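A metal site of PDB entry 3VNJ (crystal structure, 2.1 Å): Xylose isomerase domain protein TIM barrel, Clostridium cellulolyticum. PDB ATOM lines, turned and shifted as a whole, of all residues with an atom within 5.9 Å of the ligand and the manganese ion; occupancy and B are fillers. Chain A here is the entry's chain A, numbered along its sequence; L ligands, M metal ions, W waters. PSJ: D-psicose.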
ATOM      1  N   TYR A   7      13.384  15.667 -21.205  1.00  0.00           N
ATOM      2  CA  TYR A   7      13.316  14.566 -22.142  1.00  0.00           C
ATOM      3  C   TYR A   7      13.318  15.188 -23.566  1.00  0.00           C
ATOM      4  O   TYR A   7      12.526  16.094 -23.834  1.00  0.00           O
ATOM      5  CB  TYR A   7      12.048  13.779 -21.857  1.00  0.00           C
ATOM      6  CG  TYR A   7      11.894  12.445 -22.532  1.00  0.00           C
ATOM      7  CD1 TYR A   7      13.003  11.713 -22.925  1.00  0.00           C
ATOM      8  CD2 TYR A   7      10.640  11.861 -22.659  1.00  0.00           C
ATOM      9  CE1 TYR A   7      12.881  10.396 -23.438  1.00  0.00           C
ATOM     10  CE2 TYR A   7      10.478  10.530 -23.160  1.00  0.00           C
ATOM     11  CZ  TYR A   7      11.629   9.810 -23.546  1.00  0.00           C
ATOM     12  OH  TYR A   7      11.516   8.518 -24.006  1.00  0.00           O
ATOM     13  N   TRP A  15      10.087   8.045 -31.114  1.00  0.00           N
ATOM     14  CA  TRP A  15      10.974   7.666 -30.016  1.00  0.00           C
ATOM     15  C   TRP A  15      12.446   7.549 -30.440  1.00  0.00           C
ATOM     16  O   TRP A  15      13.140   6.589 -30.099  1.00  0.00           O
ATOM     17  CB  TRP A  15      10.479   6.361 -29.337  1.00  0.00           C
ATOM     18  CG  TRP A  15       9.120   6.527 -28.695  1.00  0.00           C
ATOM     19  CD1 TRP A  15       7.990   5.810 -28.989  1.00  0.00           C
ATOM     20  CD2 TRP A  15       8.735   7.476 -27.668  1.00  0.00           C
ATOM     21  NE1 TRP A  15       6.937   6.247 -28.229  1.00  0.00           N
ATOM     22  CE2 TRP A  15       7.358   7.271 -27.409  1.00  0.00           C
ATOM     23  CE3 TRP A  15       9.416   8.482 -26.962  1.00  0.00           C
ATOM     24  CZ2 TRP A  15       6.626   8.035 -26.467  1.00  0.00           C
ATOM     25  CZ3 TRP A  15       8.698   9.251 -26.020  1.00  0.00           C
ATOM     26  CH2 TRP A  15       7.313   9.017 -25.784  1.00  0.00           C
ATOM     27  N   GLU A  35      17.579  13.664 -21.364  1.00  0.00           N
ATOM     28  CA  GLU A  35      17.156  12.260 -21.267  1.00  0.00           C
ATOM     29  C   GLU A  35      16.804  11.877 -22.685  1.00  0.00           C
ATOM     30  O   GLU A  35      16.152  12.650 -23.414  1.00  0.00           O
ATOM     31  CB  GLU A  35      15.944  12.090 -20.351  1.00  0.00           C
ATOM     32  CG  GLU A  35      15.475  10.603 -20.190  1.00  0.00           C
ATOM     33  CD  GLU A  35      14.775  10.356 -18.819  1.00  0.00           C
ATOM     34  OE1 GLU A  35      15.395  10.702 -17.789  1.00  0.00           O
ATOM     35  OE2 GLU A  35      13.642   9.811 -18.800  1.00  0.00           O
ATOM     36  N   ALA A  37      15.579   8.635 -25.550  1.00  0.00           N
ATOM     37  CA  ALA A  37      14.861   7.357 -25.667  1.00  0.00           C
ATOM     38  C   ALA A  37      15.859   6.252 -26.034  1.00  0.00           C
ATOM     39  O   ALA A  37      16.782   6.477 -26.860  1.00  0.00           O
ATOM     40  CB  ALA A  37      13.768   7.448 -26.761  1.00  0.00           C
ATOM     41  N   GLY A  66      15.357   6.795 -20.975  1.00  0.00           N
ATOM     42  CA  GLY A  66      14.007   6.390 -20.661  1.00  0.00           C
ATOM     43  C   GLY A  66      13.668   5.315 -21.684  1.00  0.00           C
ATOM     44  O   GLY A  66      14.178   5.351 -22.811  1.00  0.00           O
ATOM     45  N   HIS A  67      12.833   4.337 -21.325  1.00  0.00           N
ATOM     46  CA  HIS A  67      12.427   3.317 -22.296  1.00  0.00           C
ATOM     47  C   HIS A  67      11.002   2.787 -22.061  1.00  0.00           C
ATOM     48  O   HIS A  67      10.668   2.353 -20.952  1.00  0.00           O
ATOM     49  CB  HIS A  67      13.412   2.113 -22.299  1.00  0.00           C
ATOM     50  CG  HIS A  67      13.148   1.142 -23.418  1.00  0.00           C
ATOM     51  ND1 HIS A  67      12.954   1.552 -24.719  1.00  0.00           N
ATOM     52  CD2 HIS A  67      13.043  -0.209 -23.432  1.00  0.00           C
ATOM     53  CE1 HIS A  67      12.743   0.504 -25.487  1.00  0.00           C
ATOM     54  NE2 HIS A  67      12.791  -0.584 -24.736  1.00  0.00           N
ATOM     55  N   GLY A  68      10.141   2.885 -23.061  1.00  0.00           N
ATOM     56  CA  GLY A  68       8.814   2.309 -22.919  1.00  0.00           C
ATOM     57  C   GLY A  68       9.020   0.981 -23.652  1.00  0.00           C
ATOM     58  O   GLY A  68       9.099   1.002 -24.877  1.00  0.00           O
ATOM     59  N   GLY A 106      15.245   4.274 -17.062  1.00  0.00           N
ATOM     60  CA  GLY A 106      14.001   4.258 -16.308  1.00  0.00           C
ATOM     61  C   GLY A 106      12.799   4.131 -17.196  1.00  0.00           C
ATOM     62  O   GLY A 106      12.891   4.328 -18.423  1.00  0.00           O
ATOM     63  N   GLY A 107      11.659   3.832 -16.594  1.00  0.00           N
ATOM     64  CA  GLY A 107      10.418   3.660 -17.352  1.00  0.00           C
ATOM     65  C   GLY A 107       9.717   2.396 -16.833  1.00  0.00           C
ATOM     66  O   GLY A 107      10.024   1.929 -15.740  1.00  0.00           O
ATOM     67  N   ALA A 108       8.788   1.821 -17.602  1.00  0.00           N
ATOM     68  CA  ALA A 108       8.078   0.623 -17.146  1.00  0.00           C
ATOM     69  C   ALA A 108       8.946  -0.586 -17.483  1.00  0.00           C
ATOM     70  O   ALA A 108       8.530  -1.470 -18.226  1.00  0.00           O
ATOM     71  CB  ALA A 108       6.746   0.518 -17.838  1.00  0.00           C
ATOM     72  N   TRP A 113       5.095  -0.986 -22.511  1.00  0.00           N
ATOM     73  CA  TRP A 113       4.303   0.241 -22.510  1.00  0.00           C
ATOM     74  C   TRP A 113       4.264   0.782 -23.930  1.00  0.00           C
ATOM     75  O   TRP A 113       5.292   0.862 -24.599  1.00  0.00           O
ATOM     76  CB  TRP A 113       5.016   1.287 -21.641  1.00  0.00           C
ATOM     77  CG  TRP A 113       4.422   2.683 -21.668  1.00  0.00           C
ATOM     78  CD1 TRP A 113       3.476   3.193 -20.817  1.00  0.00           C
ATOM     79  CD2 TRP A 113       4.712   3.730 -22.612  1.00  0.00           C
ATOM     80  NE1 TRP A 113       3.155   4.477 -21.161  1.00  0.00           N
ATOM     81  CE2 TRP A 113       3.902   4.850 -22.259  1.00  0.00           C
ATOM     82  CE3 TRP A 113       5.570   3.840 -23.718  1.00  0.00           C
ATOM     83  CZ2 TRP A 113       3.926   6.069 -22.981  1.00  0.00           C
ATOM     84  CZ3 TRP A 113       5.598   5.069 -24.449  1.00  0.00           C
ATOM     85  CH2 TRP A 113       4.776   6.159 -24.068  1.00  0.00           C
ATOM     86  N   GLU A 151       9.442   2.888 -12.899  1.00  0.00           N
ATOM     87  CA  GLU A 151       8.504   3.995 -12.840  1.00  0.00           C
ATOM     88  C   GLU A 151       7.093   3.621 -12.517  1.00  0.00           C
ATOM     89  O   GLU A 151       6.482   2.801 -13.177  1.00  0.00           O
ATOM     90  CB  GLU A 151       8.503   4.781 -14.164  1.00  0.00           C
ATOM     91  CG  GLU A 151       7.527   5.950 -14.206  1.00  0.00           C
ATOM     92  CD  GLU A 151       7.704   6.810 -15.506  1.00  0.00           C
ATOM     93  OE1 GLU A 151       8.359   6.382 -16.465  1.00  0.00           O
ATOM     94  OE2 GLU A 151       7.171   7.914 -15.560  1.00  0.00           O
ATOM     95  N   LEU A 153       3.374   4.148 -12.715  1.00  0.00           N
ATOM     96  CA  LEU A 153       2.521   4.763 -13.718  1.00  0.00           C
ATOM     97  C   LEU A 153       1.074   4.724 -13.355  1.00  0.00           C
ATOM     98  O   LEU A 153       0.678   3.908 -12.487  1.00  0.00           O
ATOM     99  CB  LEU A 153       2.680   4.024 -15.036  1.00  0.00           C
ATOM    100  CG  LEU A 153       4.091   3.929 -15.644  1.00  0.00           C
ATOM    101  CD1 LEU A 153       3.989   3.084 -16.883  1.00  0.00           C
ATOM    102  CD2 LEU A 153       4.618   5.298 -16.016  1.00  0.00           C
ATOM    103  N   ASN A 154       0.252   5.549 -14.023  1.00  0.00           N
ATOM    104  CA  ASN A 154      -1.155   5.537 -13.720  1.00  0.00           C
ATOM    105  C   ASN A 154      -1.802   4.292 -14.355  1.00  0.00           C
ATOM    106  O   ASN A 154      -1.254   3.646 -15.269  1.00  0.00           O
ATOM    107  CB  ASN A 154      -1.832   6.827 -14.196  1.00  0.00           C
ATOM    108  CG  ASN A 154      -1.882   6.938 -15.704  1.00  0.00           C
ATOM    109  OD1 ASN A 154      -2.613   6.193 -16.366  1.00  0.00           O
ATOM    110  ND2 ASN A 154      -1.083   7.882 -16.277  1.00  0.00           N
ATOM    111  N   GLU A 157      -2.025   3.283 -18.136  1.00  0.00           N
ATOM    112  CA  GLU A 157      -0.807   2.937 -18.869  1.00  0.00           C
ATOM    113  C   GLU A 157      -0.166   1.636 -18.451  1.00  0.00           C
ATOM    114  O   GLU A 157       0.607   1.052 -19.205  1.00  0.00           O
ATOM    115  CB  GLU A 157       0.190   4.102 -18.766  1.00  0.00           C
ATOM    116  CG  GLU A 157      -0.332   5.337 -19.472  1.00  0.00           C
ATOM    117  CD  GLU A 157       0.664   6.489 -19.492  1.00  0.00           C
ATOM    118  OE1 GLU A 157       1.879   6.284 -19.794  1.00  0.00           O
ATOM    119  OE2 GLU A 157       0.214   7.614 -19.187  1.00  0.00           O
ATOM    120  N   MET A 182      10.826   5.009  -9.185  1.00  0.00           N
ATOM    121  CA  MET A 182      10.880   6.271  -9.935  1.00  0.00           C
ATOM    122  C   MET A 182       9.466   6.783  -9.925  1.00  0.00           C
ATOM    123  O   MET A 182       8.551   6.041 -10.209  1.00  0.00           O
ATOM    124  CB  MET A 182      11.365   6.011 -11.356  1.00  0.00           C
ATOM    125  CG  MET A 182      11.097   7.070 -12.436  1.00  0.00           C
ATOM    126  SD  MET A 182      11.894   6.461 -13.982  1.00  0.00           S
ATOM    127  CE  MET A 182      11.245   7.790 -15.213  1.00  0.00           C
ATOM    128  N   ASP A 184       6.684  10.141 -10.988  1.00  0.00           N
ATOM    129  CA  ASP A 184       6.450  11.091 -12.063  1.00  0.00           C
ATOM    130  C   ASP A 184       5.211  11.889 -11.631  1.00  0.00           C
ATOM    131  O   ASP A 184       4.158  11.323 -11.440  1.00  0.00           O
ATOM    132  CB  ASP A 184       6.158  10.281 -13.333  1.00  0.00           C
ATOM    133  CG  ASP A 184       5.679  11.119 -14.522  1.00  0.00           C
ATOM    134  OD1 ASP A 184       4.911  12.128 -14.357  1.00  0.00           O
ATOM    135  OD2 ASP A 184       6.028  10.696 -15.658  1.00  0.00           O
ATOM    136  N   PHE A 186       3.054  13.562 -13.147  1.00  0.00           N
ATOM    137  CA  PHE A 186       1.831  13.397 -13.967  1.00  0.00           C
ATOM    138  C   PHE A 186       1.046  12.105 -13.545  1.00  0.00           C
ATOM    139  O   PHE A 186      -0.193  12.082 -13.540  1.00  0.00           O
ATOM    140  CB  PHE A 186       2.188  13.302 -15.460  1.00  0.00           C
ATOM    141  CG  PHE A 186       1.076  12.774 -16.329  1.00  0.00           C
ATOM    142  CD1 PHE A 186      -0.035  13.579 -16.634  1.00  0.00           C
ATOM    143  CD2 PHE A 186       1.129  11.489 -16.843  1.00  0.00           C
ATOM    144  CE1 PHE A 186      -1.041  13.104 -17.425  1.00  0.00           C
ATOM    145  CE2 PHE A 186       0.136  10.995 -17.637  1.00  0.00           C
ATOM    146  CZ  PHE A 186      -0.978  11.835 -17.927  1.00  0.00           C
ATOM    147  N   HIS A 187       1.780  11.065 -13.187  1.00  0.00           N
ATOM    148  CA  HIS A 187       1.181   9.791 -12.799  1.00  0.00           C
ATOM    149  C   HIS A 187       0.728   9.813 -11.317  1.00  0.00           C
ATOM    150  O   HIS A 187      -0.309   9.263 -10.993  1.00  0.00           O
ATOM    151  CB  HIS A 187       2.156   8.654 -13.046  1.00  0.00           C
ATOM    152  CG  HIS A 187       2.464   8.435 -14.499  1.00  0.00           C
ATOM    153  ND1 HIS A 187       1.518   8.013 -15.390  1.00  0.00           N
ATOM    154  CD2 HIS A 187       3.608   8.615 -15.206  1.00  0.00           C
ATOM    155  CE1 HIS A 187       2.051   7.918 -16.594  1.00  0.00           C
ATOM    156  NE2 HIS A 187       3.329   8.277 -16.514  1.00  0.00           N
ATOM    157  N   HIS A 210      10.425  12.256 -12.693  1.00  0.00           N
ATOM    158  CA  HIS A 210       9.971  12.891 -13.928  1.00  0.00           C
ATOM    159  C   HIS A 210       8.971  14.008 -13.539  1.00  0.00           C
ATOM    160  O   HIS A 210       8.112  13.824 -12.654  1.00  0.00           O
ATOM    161  CB  HIS A 210       9.211  11.905 -14.796  1.00  0.00           C
ATOM    162  CG  HIS A 210      10.037  11.115 -15.780  1.00  0.00           C
ATOM    163  ND1 HIS A 210       9.481  10.128 -16.564  1.00  0.00           N
ATOM    164  CD2 HIS A 210      11.349  11.144 -16.093  1.00  0.00           C
ATOM    165  CE1 HIS A 210      10.425   9.589 -17.316  1.00  0.00           C
ATOM    166  NE2 HIS A 210      11.565  10.178 -17.048  1.00  0.00           N
ATOM    167  N   ARG A 216       0.425  17.529 -18.656  1.00  0.00           N
ATOM    168  CA  ARG A 216       1.770  17.412 -19.251  1.00  0.00           C
ATOM    169  C   ARG A 216       2.439  18.630 -19.833  1.00  0.00           C
ATOM    170  O   ARG A 216       3.334  18.496 -20.657  1.00  0.00           O
ATOM    171  CB  ARG A 216       1.813  16.319 -20.317  1.00  0.00           C
ATOM    172  CG  ARG A 216       1.333  14.931 -19.871  1.00  0.00           C
ATOM    173  CD  ARG A 216       2.553  14.051 -19.483  1.00  0.00           C
ATOM    174  NE  ARG A 216       2.227  12.719 -19.860  1.00  0.00           N
ATOM    175  CZ  ARG A 216       2.940  11.640 -19.585  1.00  0.00           C
ATOM    176  NH1 ARG A 216       4.070  11.706 -18.901  1.00  0.00           N
ATOM    177  NH2 ARG A 216       2.482  10.485 -20.022  1.00  0.00           N
ATOM    178  N   GLU A 245       9.326  16.193 -18.368  1.00  0.00           N
ATOM    179  CA  GLU A 245       8.941  15.389 -19.508  1.00  0.00           C
ATOM    180  C   GLU A 245       7.667  16.031 -20.131  1.00  0.00           C
ATOM    181  O   GLU A 245       6.605  15.416 -20.147  1.00  0.00           O
ATOM    182  CB  GLU A 245       8.652  13.973 -18.970  1.00  0.00           C
ATOM    183  CG  GLU A 245       8.573  12.874 -19.996  1.00  0.00           C
ATOM    184  CD  GLU A 245       8.281  11.506 -19.330  1.00  0.00           C
ATOM    185  OE1 GLU A 245       7.487  11.476 -18.392  1.00  0.00           O
ATOM    186  OE2 GLU A 245       8.849  10.485 -19.754  1.00  0.00           O
ATOM    187  N   PHE A 247       4.865  17.087 -22.827  1.00  0.00           N
ATOM    188  CA  PHE A 247       4.398  16.529 -24.094  1.00  0.00           C
ATOM    189  C   PHE A 247       3.269  17.474 -24.482  1.00  0.00           C
ATOM    190  O   PHE A 247       2.143  17.377 -23.959  1.00  0.00           O
ATOM    191  CB  PHE A 247       3.841  15.102 -23.969  1.00  0.00           C
ATOM    192  CG  PHE A 247       4.882  14.027 -23.649  1.00  0.00           C
ATOM    193  CD1 PHE A 247       5.751  13.578 -24.628  1.00  0.00           C
ATOM    194  CD2 PHE A 247       4.973  13.491 -22.375  1.00  0.00           C
ATOM    195  CE1 PHE A 247       6.744  12.600 -24.354  1.00  0.00           C
ATOM    196  CE2 PHE A 247       5.946  12.533 -22.076  1.00  0.00           C
ATOM    197  CZ  PHE A 247       6.844  12.083 -23.088  1.00  0.00           C
ATOM    198  N   ILE A 258       1.243   8.993 -26.029  1.00  0.00           N
ATOM    199  CA  ILE A 258       1.000   9.882 -24.899  1.00  0.00           C
ATOM    200  C   ILE A 258      -0.436  10.394 -24.888  1.00  0.00           C
ATOM    201  O   ILE A 258      -0.897  10.943 -23.890  1.00  0.00           O
ATOM    202  CB  ILE A 258       2.027  11.052 -24.929  1.00  0.00           C
ATOM    203  CG1 ILE A 258       3.430  10.446 -24.827  1.00  0.00           C
ATOM    204  CG2 ILE A 258       1.776  12.058 -23.806  1.00  0.00           C
ATOM    205  CD1 ILE A 258       3.770   9.838 -23.450  1.00  0.00           C
HETATM  206  C1  PSJ L   1       4.954   7.591 -19.993  1.00  0.00           C
HETATM  207  O1  PSJ L   1       3.657   8.025 -19.588  1.00  0.00           O
HETATM  208  C2  PSJ L   1       6.006   8.002 -18.950  1.00  0.00           C
HETATM  209  O2  PSJ L   1       5.824   8.869 -18.121  1.00  0.00           O
HETATM  210  C3  PSJ L   1       7.299   7.167 -18.946  1.00  0.00           C
HETATM  211  O3  PSJ L   1       8.371   8.050 -18.629  1.00  0.00           O
HETATM  212  C4  PSJ L   1       7.549   6.506 -20.303  1.00  0.00           C
HETATM  213  O4  PSJ L   1       8.454   5.413 -20.156  1.00  0.00           O
HETATM  214  C5  PSJ L   1       8.204   7.498 -21.273  1.00  0.00           C
HETATM  215  O5  PSJ L   1       7.396   8.663 -21.409  1.00  0.00           O
HETATM  216  C6  PSJ L   1       8.371   6.755 -22.602  1.00  0.00           C
HETATM  217  O6  PSJ L   1       9.216   7.481 -23.496  1.00  0.00           O
HETATM  218 MN    MN M   1       7.422   9.615 -16.942  1.00  0.00          MN
HETATM  219  O   HOH W   1      10.118   5.031 -25.310  1.00  0.00           O
HETATM  220  O   HOH W   2      10.852   6.396 -19.186  1.00  0.00           O
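CZ3 of Trp 15 touches O6 of the ligand, at 3.1 Å.
O of His 67 touches O4 of the ligand, at 3.9 Å.
Gly 107 touches the ligand.
Trp 113 touches the ligand.
Phe 247 touches the ligand.
Hydrophobic or aromatic side chains that line the ligand: Tyr 7, Trp 15, Trp 113, His 187, His 210 and Phe 247.
13 residues have an atom within 4 Å of the ligand: Tyr 7, Trp 15, His 67, Gly 107, Trp 113, Glu 151, Glu 157, Asp 184, His 187, His 210, Arg 216, Glu 245 and Phe 247.
The nearest printed residue that does not touch the ligand is Gly 68 (4.2 Å).
Water W2 bridges an oxygen (O4) of the ligand (2.8 Å) and the backbone carbonyl oxygen (O) of Gly 106 (3.0 Å).
Water W1 bridges the backbone NH of Gly 68 (3.1 Å) and an oxygen (O6) of the ligand (3.2 Å).
Within 4 Å of the manganese ion: Glu 151, Asp 184, His 210 and Glu 245.
A ring nitrogen (NE2) of His 187 sits at hydrogen-bond distance from an oxygen (O1) of the ligand, at 3.1 Å.
The guanidinium group (NH2) of Arg 216 sits at hydrogen-bond distance from an oxygen (O1) of the ligand, 2.8 Å away.
An oxygen (O1) of the ligand sits at hydrogen-bond distance from the side-chain carboxylate (OE1) of Glu 157 (2.5 Å).
An oxygen (O6) of the ligand sits at hydrogen-bond distance from the side-chain hydroxyl (OH) of Tyr 7 (2.6 Å).
The manganese ion is bound by O2 of the ligand (2.1 Å).
ND1 of His 210 is bound to the manganese ion, at 2.2 Å.
The side-chain carboxylate (OD2) of Asp 184 binds the manganese ion, at 2.2 Å.
OE2 of Glu 151 binds the manganese ion (2.2 Å).
OE1 of Glu 245 binds the manganese ion (2.4 Å).
O3 of the ligand binds the manganese ion (2.5 Å).
NH1 of Arg 216 sits close to OD2 of Asp 184 (3.9 Å).
The backbone NH (N) of Phe 186 is in hydrogen-bond range of the side-chain carboxylate (OD1) of Asp 184, 2.6 Å away.
The backbone carbonyl oxygen (O) of Gly 106 lies within hydrogen-bond range of the backbone NH (N) of His 67 (2.9 Å).
The side-chain carboxylate (OE2) of Glu 157 is in hydrogen-bond range of the side-chain amide nitrogen (ND2) of Asn 154 (3.2 Å).
NE2 of His 210 lies within hydrogen-bond range of OE2 of Glu 35.
The backbone carbonyl oxygen of Arg 216 lies within hydrogen-bond range of the backbone NH of Phe 247 (3.0 Å).
A ring nitrogen (ND1) of His 187 sits at hydrogen-bond distance from the side-chain amide nitrogen (ND2) of Asn 154.
The backbone NH (N) of Gly 107 sits at hydrogen-bond distance from the side-chain sulfur (SD) of Met 182 (3.7 Å).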
